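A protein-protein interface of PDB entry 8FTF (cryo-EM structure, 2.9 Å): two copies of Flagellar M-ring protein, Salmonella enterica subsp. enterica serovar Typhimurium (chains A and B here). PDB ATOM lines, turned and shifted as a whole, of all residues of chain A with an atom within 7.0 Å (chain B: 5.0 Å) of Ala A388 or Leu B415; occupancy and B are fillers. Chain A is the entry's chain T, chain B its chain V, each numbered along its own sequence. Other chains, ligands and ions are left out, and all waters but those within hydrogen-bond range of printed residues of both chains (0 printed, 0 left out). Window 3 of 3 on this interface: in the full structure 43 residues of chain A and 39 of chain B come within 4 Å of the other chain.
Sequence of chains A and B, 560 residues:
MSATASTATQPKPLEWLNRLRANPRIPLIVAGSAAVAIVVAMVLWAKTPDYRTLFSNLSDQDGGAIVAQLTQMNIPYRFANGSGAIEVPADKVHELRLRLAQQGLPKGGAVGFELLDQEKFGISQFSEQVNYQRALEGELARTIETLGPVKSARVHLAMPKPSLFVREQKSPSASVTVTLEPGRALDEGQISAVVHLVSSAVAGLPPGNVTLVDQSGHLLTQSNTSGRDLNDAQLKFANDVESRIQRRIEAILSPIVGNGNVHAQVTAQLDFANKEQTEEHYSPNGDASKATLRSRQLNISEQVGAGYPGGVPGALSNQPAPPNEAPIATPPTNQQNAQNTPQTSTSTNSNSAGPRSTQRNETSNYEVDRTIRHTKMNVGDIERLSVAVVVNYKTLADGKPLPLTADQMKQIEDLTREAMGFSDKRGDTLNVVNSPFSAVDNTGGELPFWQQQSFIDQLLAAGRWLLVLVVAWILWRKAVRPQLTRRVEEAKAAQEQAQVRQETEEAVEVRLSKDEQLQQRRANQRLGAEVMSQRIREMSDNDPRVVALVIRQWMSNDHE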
ATOM      1  N   HIS A 263       1.872  13.289  -7.617  1.00  0.00           N
ATOM      2  CA  HIS A 263       1.018  14.432  -7.326  1.00  0.00           C
ATOM      3  C   HIS A 263       1.521  15.631  -8.115  1.00  0.00           C
ATOM      4  O   HIS A 263       2.732  15.868  -8.179  1.00  0.00           O
ATOM      5  CB  HIS A 263       1.001  14.750  -5.827  1.00  0.00           C
ATOM      6  CG  HIS A 263       0.078  13.877  -5.034  1.00  0.00           C
ATOM      7  ND1 HIS A 263      -1.293  14.014  -5.075  1.00  0.00           N
ATOM      8  CD2 HIS A 263       0.330  12.858  -4.180  1.00  0.00           C
ATOM      9  CE1 HIS A 263      -1.846  13.115  -4.281  1.00  0.00           C
ATOM     10  NE2 HIS A 263      -0.884  12.402  -3.725  1.00  0.00           N
ATOM     11  N   ALA A 264       0.599  16.382  -8.711  1.00  0.00           N
ATOM     12  CA  ALA A 264       0.954  17.535  -9.526  1.00  0.00           C
ATOM     13  C   ALA A 264      -0.044  18.658  -9.302  1.00  0.00           C
ATOM     14  O   ALA A 264      -1.249  18.417  -9.190  1.00  0.00           O
ATOM     15  CB  ALA A 264       1.004  17.171 -11.015  1.00  0.00           C
ATOM     16  N   GLN A 265       0.466  19.886  -9.237  1.00  0.00           N
ATOM     17  CA  GLN A 265      -0.358  21.082  -9.101  1.00  0.00           C
ATOM     18  C   GLN A 265       0.041  22.077 -10.179  1.00  0.00           C
ATOM     19  O   GLN A 265       1.233  22.287 -10.422  1.00  0.00           O
ATOM     20  CB  GLN A 265      -0.206  21.708  -7.710  1.00  0.00           C
ATOM     21  N   VAL A 266      -0.954  22.686 -10.819  1.00  0.00           N
ATOM     22  CA  VAL A 266      -0.742  23.586 -11.946  1.00  0.00           C
ATOM     23  C   VAL A 266      -1.386  24.930 -11.633  1.00  0.00           C
ATOM     24  O   VAL A 266      -2.535  24.982 -11.181  1.00  0.00           O
ATOM     25  CB  VAL A 266      -1.314  23.005 -13.254  1.00  0.00           C
ATOM     26  CG1 VAL A 266      -0.870  23.839 -14.444  1.00  0.00           C
ATOM     27  CG2 VAL A 266      -0.891  21.555 -13.426  1.00  0.00           C
ATOM     28  N   THR A 267      -0.644  26.008 -11.872  1.00  0.00           N
ATOM     29  CA  THR A 267      -1.157  27.367 -11.767  1.00  0.00           C
ATOM     30  C   THR A 267      -1.052  28.031 -13.134  1.00  0.00           C
ATOM     31  O   THR A 267      -0.088  27.796 -13.870  1.00  0.00           O
ATOM     32  CB  THR A 267      -0.397  28.175 -10.705  1.00  0.00           C
ATOM     33  OG1 THR A 267      -0.981  29.479 -10.583  1.00  0.00           O
ATOM     34  CG2 THR A 267       1.078  28.309 -11.061  1.00  0.00           C
ATOM     35  N   SER A 386       3.069  27.188 -14.661  1.00  0.00           N
ATOM     36  CA  SER A 386       4.041  26.674 -13.706  1.00  0.00           C
ATOM     37  C   SER A 386       3.492  25.400 -13.080  1.00  0.00           C
ATOM     38  O   SER A 386       2.369  25.393 -12.567  1.00  0.00           O
ATOM     39  CB  SER A 386       4.357  27.709 -12.622  1.00  0.00           C
ATOM     40  OG  SER A 386       4.982  28.853 -13.176  1.00  0.00           O
ATOM     41  N   VAL A 387       4.283  24.331 -13.124  1.00  0.00           N
ATOM     42  CA  VAL A 387       3.867  23.018 -12.644  1.00  0.00           C
ATOM     43  C   VAL A 387       4.929  22.471 -11.702  1.00  0.00           C
ATOM     44  O   VAL A 387       6.130  22.565 -11.983  1.00  0.00           O
ATOM     45  CB  VAL A 387       3.624  22.036 -13.812  1.00  0.00           C
ATOM     46  CG1 VAL A 387       3.162  20.685 -13.290  1.00  0.00           C
ATOM     47  CG2 VAL A 387       2.607  22.609 -14.786  1.00  0.00           C
ATOM     48  N   ALA A 388       4.487  21.899 -10.583  1.00  0.00           N
ATOM     49  CA  ALA A 388       5.367  21.242  -9.628  1.00  0.00           C
ATOM     50  C   ALA A 388       4.894  19.809  -9.435  1.00  0.00           C
ATOM     51  O   ALA A 388       3.703  19.569  -9.218  1.00  0.00           O
ATOM     52  CB  ALA A 388       5.389  21.982  -8.288  1.00  0.00           C
ATOM     53  N   VAL A 389       5.827  18.862  -9.513  1.00  0.00           N
ATOM     54  CA  VAL A 389       5.518  17.437  -9.464  1.00  0.00           C
ATOM     55  C   VAL A 389       6.424  16.769  -8.442  1.00  0.00           C
ATOM     56  O   VAL A 389       7.631  17.035  -8.400  1.00  0.00           O
ATOM     57  CB  VAL A 389       5.678  16.774 -10.851  1.00  0.00           C
ATOM     58  CG1 VAL A 389       5.429  15.276 -10.764  1.00  0.00           C
ATOM     59  CG2 VAL A 389       4.738  17.414 -11.861  1.00  0.00           C
ATOM     60  N   VAL A 390       5.842  15.903  -7.616  1.00  0.00           N
ATOM     61  CA  VAL A 390       6.569  15.149  -6.602  1.00  0.00           C
ATOM     62  C   VAL A 390       6.292  13.666  -6.816  1.00  0.00           C
ATOM     63  O   VAL A 390       5.154  13.277  -7.105  1.00  0.00           O
ATOM     64  CB  VAL A 390       6.178  15.584  -5.178  1.00  0.00           C
ATOM     65  CG1 VAL A 390       6.745  16.960  -4.873  1.00  0.00           C
ATOM     66  CG2 VAL A 390       4.667  15.588  -5.014  1.00  0.00           C
ATOM     67  N   THR A 429       7.897  27.439 -16.759  1.00  0.00           N
ATOM     68  CA  THR A 429       8.799  26.966 -15.718  1.00  0.00           C
ATOM     69  C   THR A 429       8.313  25.614 -15.216  1.00  0.00           C
ATOM     70  O   THR A 429       7.112  25.412 -15.020  1.00  0.00           O
ATOM     71  CB  THR A 429       8.887  27.951 -14.542  1.00  0.00           C
ATOM     72  OG1 THR A 429       7.594  28.101 -13.942  1.00  0.00           O
ATOM     73  CG2 THR A 429       9.387  29.312 -15.009  1.00  0.00           C
ATOM     74  N   LEU A 430       9.252  24.693 -15.012  1.00  0.00           N
ATOM     75  CA  LEU A 430       8.949  23.355 -14.524  1.00  0.00           C
ATOM     76  C   LEU A 430       9.950  22.977 -13.445  1.00  0.00           C
ATOM     77  O   LEU A 430      11.145  23.257 -13.577  1.00  0.00           O
ATOM     78  CB  LEU A 430       8.982  22.329 -15.664  1.00  0.00           C
ATOM     79  CG  LEU A 430       8.863  20.855 -15.276  1.00  0.00           C
ATOM     80  CD1 LEU A 430       7.408  20.467 -15.065  1.00  0.00           C
ATOM     81  CD2 LEU A 430       9.507  19.972 -16.332  1.00  0.00           C
ATOM     82  N   ASN A 431       9.461  22.344 -12.379  1.00  0.00           N
ATOM     83  CA  ASN A 431      10.300  21.893 -11.275  1.00  0.00           C
ATOM     84  C   ASN A 431       9.761  20.565 -10.766  1.00  0.00           C
ATOM     85  O   ASN A 431       8.605  20.486 -10.338  1.00  0.00           O
ATOM     86  CB  ASN A 431      10.335  22.928 -10.147  1.00  0.00           C
ATOM     87  CG  ASN A 431      11.355  22.593  -9.072  1.00  0.00           C
ATOM     88  OD1 ASN A 431      12.036  21.571  -9.140  1.00  0.00           O
ATOM     89  ND2 ASN A 431      11.465  23.461  -8.072  1.00  0.00           N
ATOM     90  N   VAL A 432      10.595  19.529 -10.813  1.00  0.00           N
ATOM     91  CA  VAL A 432      10.241  18.196 -10.342  1.00  0.00           C
ATOM     92  C   VAL A 432      11.272  17.766  -9.307  1.00  0.00           C
ATOM     93  O   VAL A 432      12.480  17.863  -9.552  1.00  0.00           O
ATOM     94  CB  VAL A 432      10.173  17.182 -11.499  1.00  0.00           C
ATOM     95  CG1 VAL A 432       9.695  15.832 -10.992  1.00  0.00           C
ATOM     96  CG2 VAL A 432       9.260  17.692 -12.604  1.00  0.00           C
ATOM     97  N   VAL A 433      10.796  17.291  -8.159  1.00  0.00           N
ATOM     98  CA  VAL A 433      11.657  16.835  -7.075  1.00  0.00           C
ATOM     99  C   VAL A 433      11.195  15.456  -6.629  1.00  0.00           C
ATOM    100  O   VAL A 433      10.006  15.130  -6.718  1.00  0.00           O
ATOM    101  CB  VAL A 433      11.658  17.821  -5.887  1.00  0.00           C
ATOM    102  CG1 VAL A 433      12.391  19.100  -6.258  1.00  0.00           C
ATOM    103  CG2 VAL A 433      10.236  18.124  -5.448  1.00  0.00           C
ATOM    104  N   SER A 435      11.197  12.794  -3.419  1.00  0.00           N
ATOM    105  CA  SER A 435      11.320  12.777  -1.968  1.00  0.00           C
ATOM    106  C   SER A 435      10.373  11.723  -1.415  1.00  0.00           C
ATOM    107  O   SER A 435       9.396  11.351  -2.079  1.00  0.00           O
ATOM    108  CB  SER A 435      11.004  14.159  -1.368  1.00  0.00           C
ATOM    109  OG  SER A 435      11.952  15.126  -1.785  1.00  0.00           O
ATOM    110  N   ILE B 252      -0.377  20.604  -2.423  1.00  0.00           N
ATOM    111  CA  ILE B 252       0.862  20.089  -2.999  1.00  0.00           C
ATOM    112  C   ILE B 252       1.831  19.653  -1.903  1.00  0.00           C
ATOM    113  O   ILE B 252       2.532  18.644  -2.043  1.00  0.00           O
ATOM    114  CB  ILE B 252       1.492  21.132  -3.943  1.00  0.00           C
ATOM    115  CG1 ILE B 252       2.787  20.594  -4.556  1.00  0.00           C
ATOM    116  CG2 ILE B 252       1.741  22.448  -3.223  1.00  0.00           C
ATOM    117  CD1 ILE B 252       2.610  19.306  -5.327  1.00  0.00           C
ATOM    118  N   LEU B 253       1.880  20.392  -0.796  1.00  0.00           N
ATOM    119  CA  LEU B 253       2.822  20.113   0.278  1.00  0.00           C
ATOM    120  C   LEU B 253       2.278  19.157   1.332  1.00  0.00           C
ATOM    121  O   LEU B 253       3.035  18.747   2.217  1.00  0.00           O
ATOM    122  CB  LEU B 253       3.249  21.420   0.959  1.00  0.00           C
ATOM    123  CG  LEU B 253       4.182  22.330   0.159  1.00  0.00           C
ATOM    124  CD1 LEU B 253       4.645  23.501   1.009  1.00  0.00           C
ATOM    125  CD2 LEU B 253       5.373  21.546  -0.368  1.00  0.00           C
ATOM    126  N   ILE B 256       4.037  15.499   1.539  1.00  0.00           N
ATOM    127  CA  ILE B 256       5.454  15.489   1.890  1.00  0.00           C
ATOM    128  C   ILE B 256       5.648  15.621   3.396  1.00  0.00           C
ATOM    129  O   ILE B 256       6.417  14.867   4.003  1.00  0.00           O
ATOM    130  CB  ILE B 256       6.202  16.596   1.124  1.00  0.00           C
ATOM    131  CG1 ILE B 256       6.246  16.268  -0.369  1.00  0.00           C
ATOM    132  CG2 ILE B 256       7.608  16.771   1.672  1.00  0.00           C
ATOM    133  CD1 ILE B 256       6.811  17.381  -1.213  1.00  0.00           C
ATOM    134  N   LYS B 410      14.791  23.666   0.698  1.00  0.00           N
ATOM    135  CA  LYS B 410      14.869  24.227  -0.648  1.00  0.00           C
ATOM    136  C   LYS B 410      13.826  23.604  -1.568  1.00  0.00           C
ATOM    137  O   LYS B 410      13.214  24.300  -2.387  1.00  0.00           O
ATOM    138  CB  LYS B 410      16.274  24.031  -1.218  1.00  0.00           C
ATOM    139  CG  LYS B 410      16.495  24.705  -2.562  1.00  0.00           C
ATOM    140  CD  LYS B 410      17.909  24.479  -3.067  1.00  0.00           C
ATOM    141  CE  LYS B 410      18.921  25.264  -2.248  1.00  0.00           C
ATOM    142  NZ  LYS B 410      18.763  26.733  -2.436  1.00  0.00           N
ATOM    143  N   GLN B 411      13.621  22.288  -1.458  1.00  0.00           N
ATOM    144  CA  GLN B 411      12.594  21.630  -2.261  1.00  0.00           C
ATOM    145  C   GLN B 411      11.207  22.173  -1.936  1.00  0.00           C
ATOM    146  O   GLN B 411      10.405  22.428  -2.841  1.00  0.00           O
ATOM    147  CB  GLN B 411      12.641  20.119  -2.041  1.00  0.00           C
ATOM    148  CG  GLN B 411      13.866  19.439  -2.626  1.00  0.00           C
ATOM    149  CD  GLN B 411      13.880  17.946  -2.365  1.00  0.00           C
ATOM    150  OE1 GLN B 411      13.118  17.441  -1.539  1.00  0.00           O
ATOM    151  NE2 GLN B 411      14.747  17.229  -3.069  1.00  0.00           N
ATOM    152  N   ILE B 412      10.910  22.352  -0.647  1.00  0.00           N
ATOM    153  CA  ILE B 412       9.615  22.898  -0.247  1.00  0.00           C
ATOM    154  C   ILE B 412       9.445  24.313  -0.784  1.00  0.00           C
ATOM    155  O   ILE B 412       8.371  24.684  -1.280  1.00  0.00           O
ATOM    156  CB  ILE B 412       9.465  22.848   1.285  1.00  0.00           C
ATOM    157  CG1 ILE B 412       9.324  21.402   1.762  1.00  0.00           C
ATOM    158  CG2 ILE B 412       8.273  23.676   1.737  1.00  0.00           C
ATOM    159  CD1 ILE B 412       9.358  21.248   3.266  1.00  0.00           C
ATOM    160  N   GLU B 413      10.500  25.128  -0.691  1.00  0.00           N
ATOM    161  CA  GLU B 413      10.437  26.490  -1.206  1.00  0.00           C
ATOM    162  C   GLU B 413      10.183  26.505  -2.706  1.00  0.00           C
ATOM    163  O   GLU B 413       9.354  27.280  -3.195  1.00  0.00           O
ATOM    164  CB  GLU B 413      11.728  27.238  -0.874  1.00  0.00           C
ATOM    165  CG  GLU B 413      11.772  28.664  -1.398  1.00  0.00           C
ATOM    166  CD  GLU B 413      13.053  29.383  -1.021  1.00  0.00           C
ATOM    167  OE1 GLU B 413      13.916  28.762  -0.366  1.00  0.00           O
ATOM    168  OE2 GLU B 413      13.196  30.572  -1.378  1.00  0.00           O
ATOM    169  N   ASP B 414      10.880  25.647  -3.455  1.00  0.00           N
ATOM    170  CA  ASP B 414      10.672  25.591  -4.899  1.00  0.00           C
ATOM    171  C   ASP B 414       9.256  25.142  -5.240  1.00  0.00           C
ATOM    172  O   ASP B 414       8.622  25.697  -6.146  1.00  0.00           O
ATOM    173  CB  ASP B 414      11.701  24.661  -5.542  1.00  0.00           C
ATOM    174  CG  ASP B 414      13.048  25.328  -5.736  1.00  0.00           C
ATOM    175  OD1 ASP B 414      13.100  26.577  -5.726  1.00  0.00           O
ATOM    176  OD2 ASP B 414      14.053  24.607  -5.896  1.00  0.00           O
ATOM    177  N   LEU B 415       8.741  24.137  -4.526  1.00  0.00           N
ATOM    178  CA  LEU B 415       7.397  23.649  -4.812  1.00  0.00           C
ATOM    179  C   LEU B 415       6.344  24.711  -4.523  1.00  0.00           C
ATOM    180  O   LEU B 415       5.426  24.919  -5.327  1.00  0.00           O
ATOM    181  CB  LEU B 415       7.111  22.381  -4.008  1.00  0.00           C
ATOM    182  CG  LEU B 415       7.890  21.137  -4.432  1.00  0.00           C
ATOM    183  CD1 LEU B 415       7.330  19.906  -3.750  1.00  0.00           C
ATOM    184  CD2 LEU B 415       7.867  20.976  -5.944  1.00  0.00           C
ATOM    185  N   THR B 416       6.459  25.407  -3.388  1.00  0.00           N
ATOM    186  CA  THR B 416       5.471  26.435  -3.079  1.00  0.00           C
ATOM    187  C   THR B 416       5.611  27.631  -4.016  1.00  0.00           C
ATOM    188  O   THR B 416       4.612  28.266  -4.370  1.00  0.00           O
ATOM    189  CB  THR B 416       5.573  26.863  -1.609  1.00  0.00           C
ATOM    190  OG1 THR B 416       4.479  27.732  -1.289  1.00  0.00           O
ATOM    191  CG2 THR B 416       6.880  27.581  -1.324  1.00  0.00           C
ATOM    192  N   ARG B 417       6.837  27.929  -4.456  1.00  0.00           N
ATOM    193  CA  ARG B 417       7.037  28.985  -5.438  1.00  0.00           C
ATOM    194  C   ARG B 417       6.349  28.651  -6.755  1.00  0.00           C
ATOM    195  O   ARG B 417       5.658  29.496  -7.336  1.00  0.00           O
ATOM    196  CB  ARG B 417       8.535  29.206  -5.652  1.00  0.00           C
ATOM    197  CG  ARG B 417       8.871  30.256  -6.680  1.00  0.00           C
ATOM    198  CD  ARG B 417      10.367  30.335  -6.919  1.00  0.00           C
ATOM    199  NE  ARG B 417      11.090  30.708  -5.710  1.00  0.00           N
ATOM    200  CZ  ARG B 417      11.985  31.685  -5.643  1.00  0.00           C
ATOM    201  NH1 ARG B 417      12.291  32.414  -6.704  1.00  0.00           N
ATOM    202  NH2 ARG B 417      12.584  31.936  -4.483  1.00  0.00           N
ATOM    203  N   GLU B 418       6.517  27.416  -7.234  1.00  0.00           N
ATOM    204  CA  GLU B 418       5.853  27.010  -8.468  1.00  0.00           C
ATOM    205  C   GLU B 418       4.339  27.000  -8.305  1.00  0.00           C
ATOM    206  O   GLU B 418       3.608  27.379  -9.229  1.00  0.00           O
ATOM    207  CB  GLU B 418       6.353  25.634  -8.911  1.00  0.00           C
ATOM    208  CG  GLU B 418       7.816  25.611  -9.317  1.00  0.00           C
ATOM    209  CD  GLU B 418       8.105  26.516 -10.497  1.00  0.00           C
ATOM    210  OE1 GLU B 418       7.365  26.443 -11.498  1.00  0.00           O
ATOM    211  OE2 GLU B 418       9.075  27.299 -10.422  1.00  0.00           O
ATOM    212  N   ALA B 419       3.849  26.566  -7.142  1.00  0.00           N
ATOM    213  CA  ALA B 419       2.410  26.544  -6.909  1.00  0.00           C
ATOM    214  C   ALA B 419       1.822  27.950  -6.898  1.00  0.00           C
ATOM    215  O   ALA B 419       0.734  28.178  -7.442  1.00  0.00           O
ATOM    216  CB  ALA B 419       2.102  25.825  -5.594  1.00  0.00           C
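The side-chain carboxylate (OE1) of Glu B418 is in hydrogen-bond range of the side-chain hydroxyl (OG1) of Thr A429 (3.0 Å).
The side-chain hydroxyl of Ser A435 is in hydrogen-bond range of the side-chain amide oxygen of Gln B411 (2.6 Å).
The backbone carbonyl oxygen (O) of His A263 sits at hydrogen-bond distance from the backbone NH (N) of Val A390, 3.2 Å away.
The backbone carbonyl oxygen (O) of Ala A388 lies within hydrogen-bond range of the backbone NH (N) of Gln A265, 3.3 Å away.
The backbone carbonyl oxygen of Ser A386 sits at hydrogen-bond distance from the backbone NH of Thr A267, at 3.2 Å.
OG of Ser A386 is in hydrogen-bond range of OG1 of Thr A429 (2.8 Å).
O of Asn A431 is in hydrogen-bond range of N of Val A389 (3.3 Å).
The backbone NH of Val A433 lies within hydrogen-bond range of the backbone carbonyl oxygen of Val A389 (3.2 Å).
Glu B418 touches Thr A267 (O to CG2, 3.3 Å).
O of Ala B419 touches CB of Thr A267, 3.5 Å away.
Glu B418 touches Ser A386.
Ala A388 touches Leu B415 (CB to CD2, 3.6 Å).
Ala A388 touches Glu B418 (CB to CB, 3.8 Å).
Ile B256 touches Val A390.
Asn A431 touches Asp B414.
Asn A431 touches Glu B418 (CB to CG, 3.8 Å).
CG of Gln B411 touches CG1 of Val A433, 3.9 Å away.
CD2 of Leu B415 touches CG2 of Val A433 (3.7 Å).
Val A266 touches none of the printed residues of chain B.
Printed residues of chain B within 4 Å of Ser A386: Glu B418 (3.5 Å).
Printed residues of chain B within 4 Å of Val A433: Gln B411 (3.9 Å) and Leu B415 (3.7 Å).
Leu B253 touches none of the printed residues of chain A.
Of the printed residues of chain A, Leu B415 touches Ala A388 (3.6 Å), Val A390 (3.2 Å) and Val A433 (3.7 Å).
The nearest residue of chain A that does not touch Leu B415 is Asn A431 (4.5 Å).
The nearest printed residue of chain B that does not touch Thr A267 is Arg B417 (6.0 Å).
Of the 13 printed residues of chain B, 6 touch a printed residue of chain A.
Hydrophobic or aromatic side chains of chain B that line the printed part of chain A: Ile B256 and Leu B415.
Along chain B the printed residues that touch a printed residue of chain A span positions 256 to 419.
Among the printed residues, 13 pairs touch across the chains.
No position is printed for both chains.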
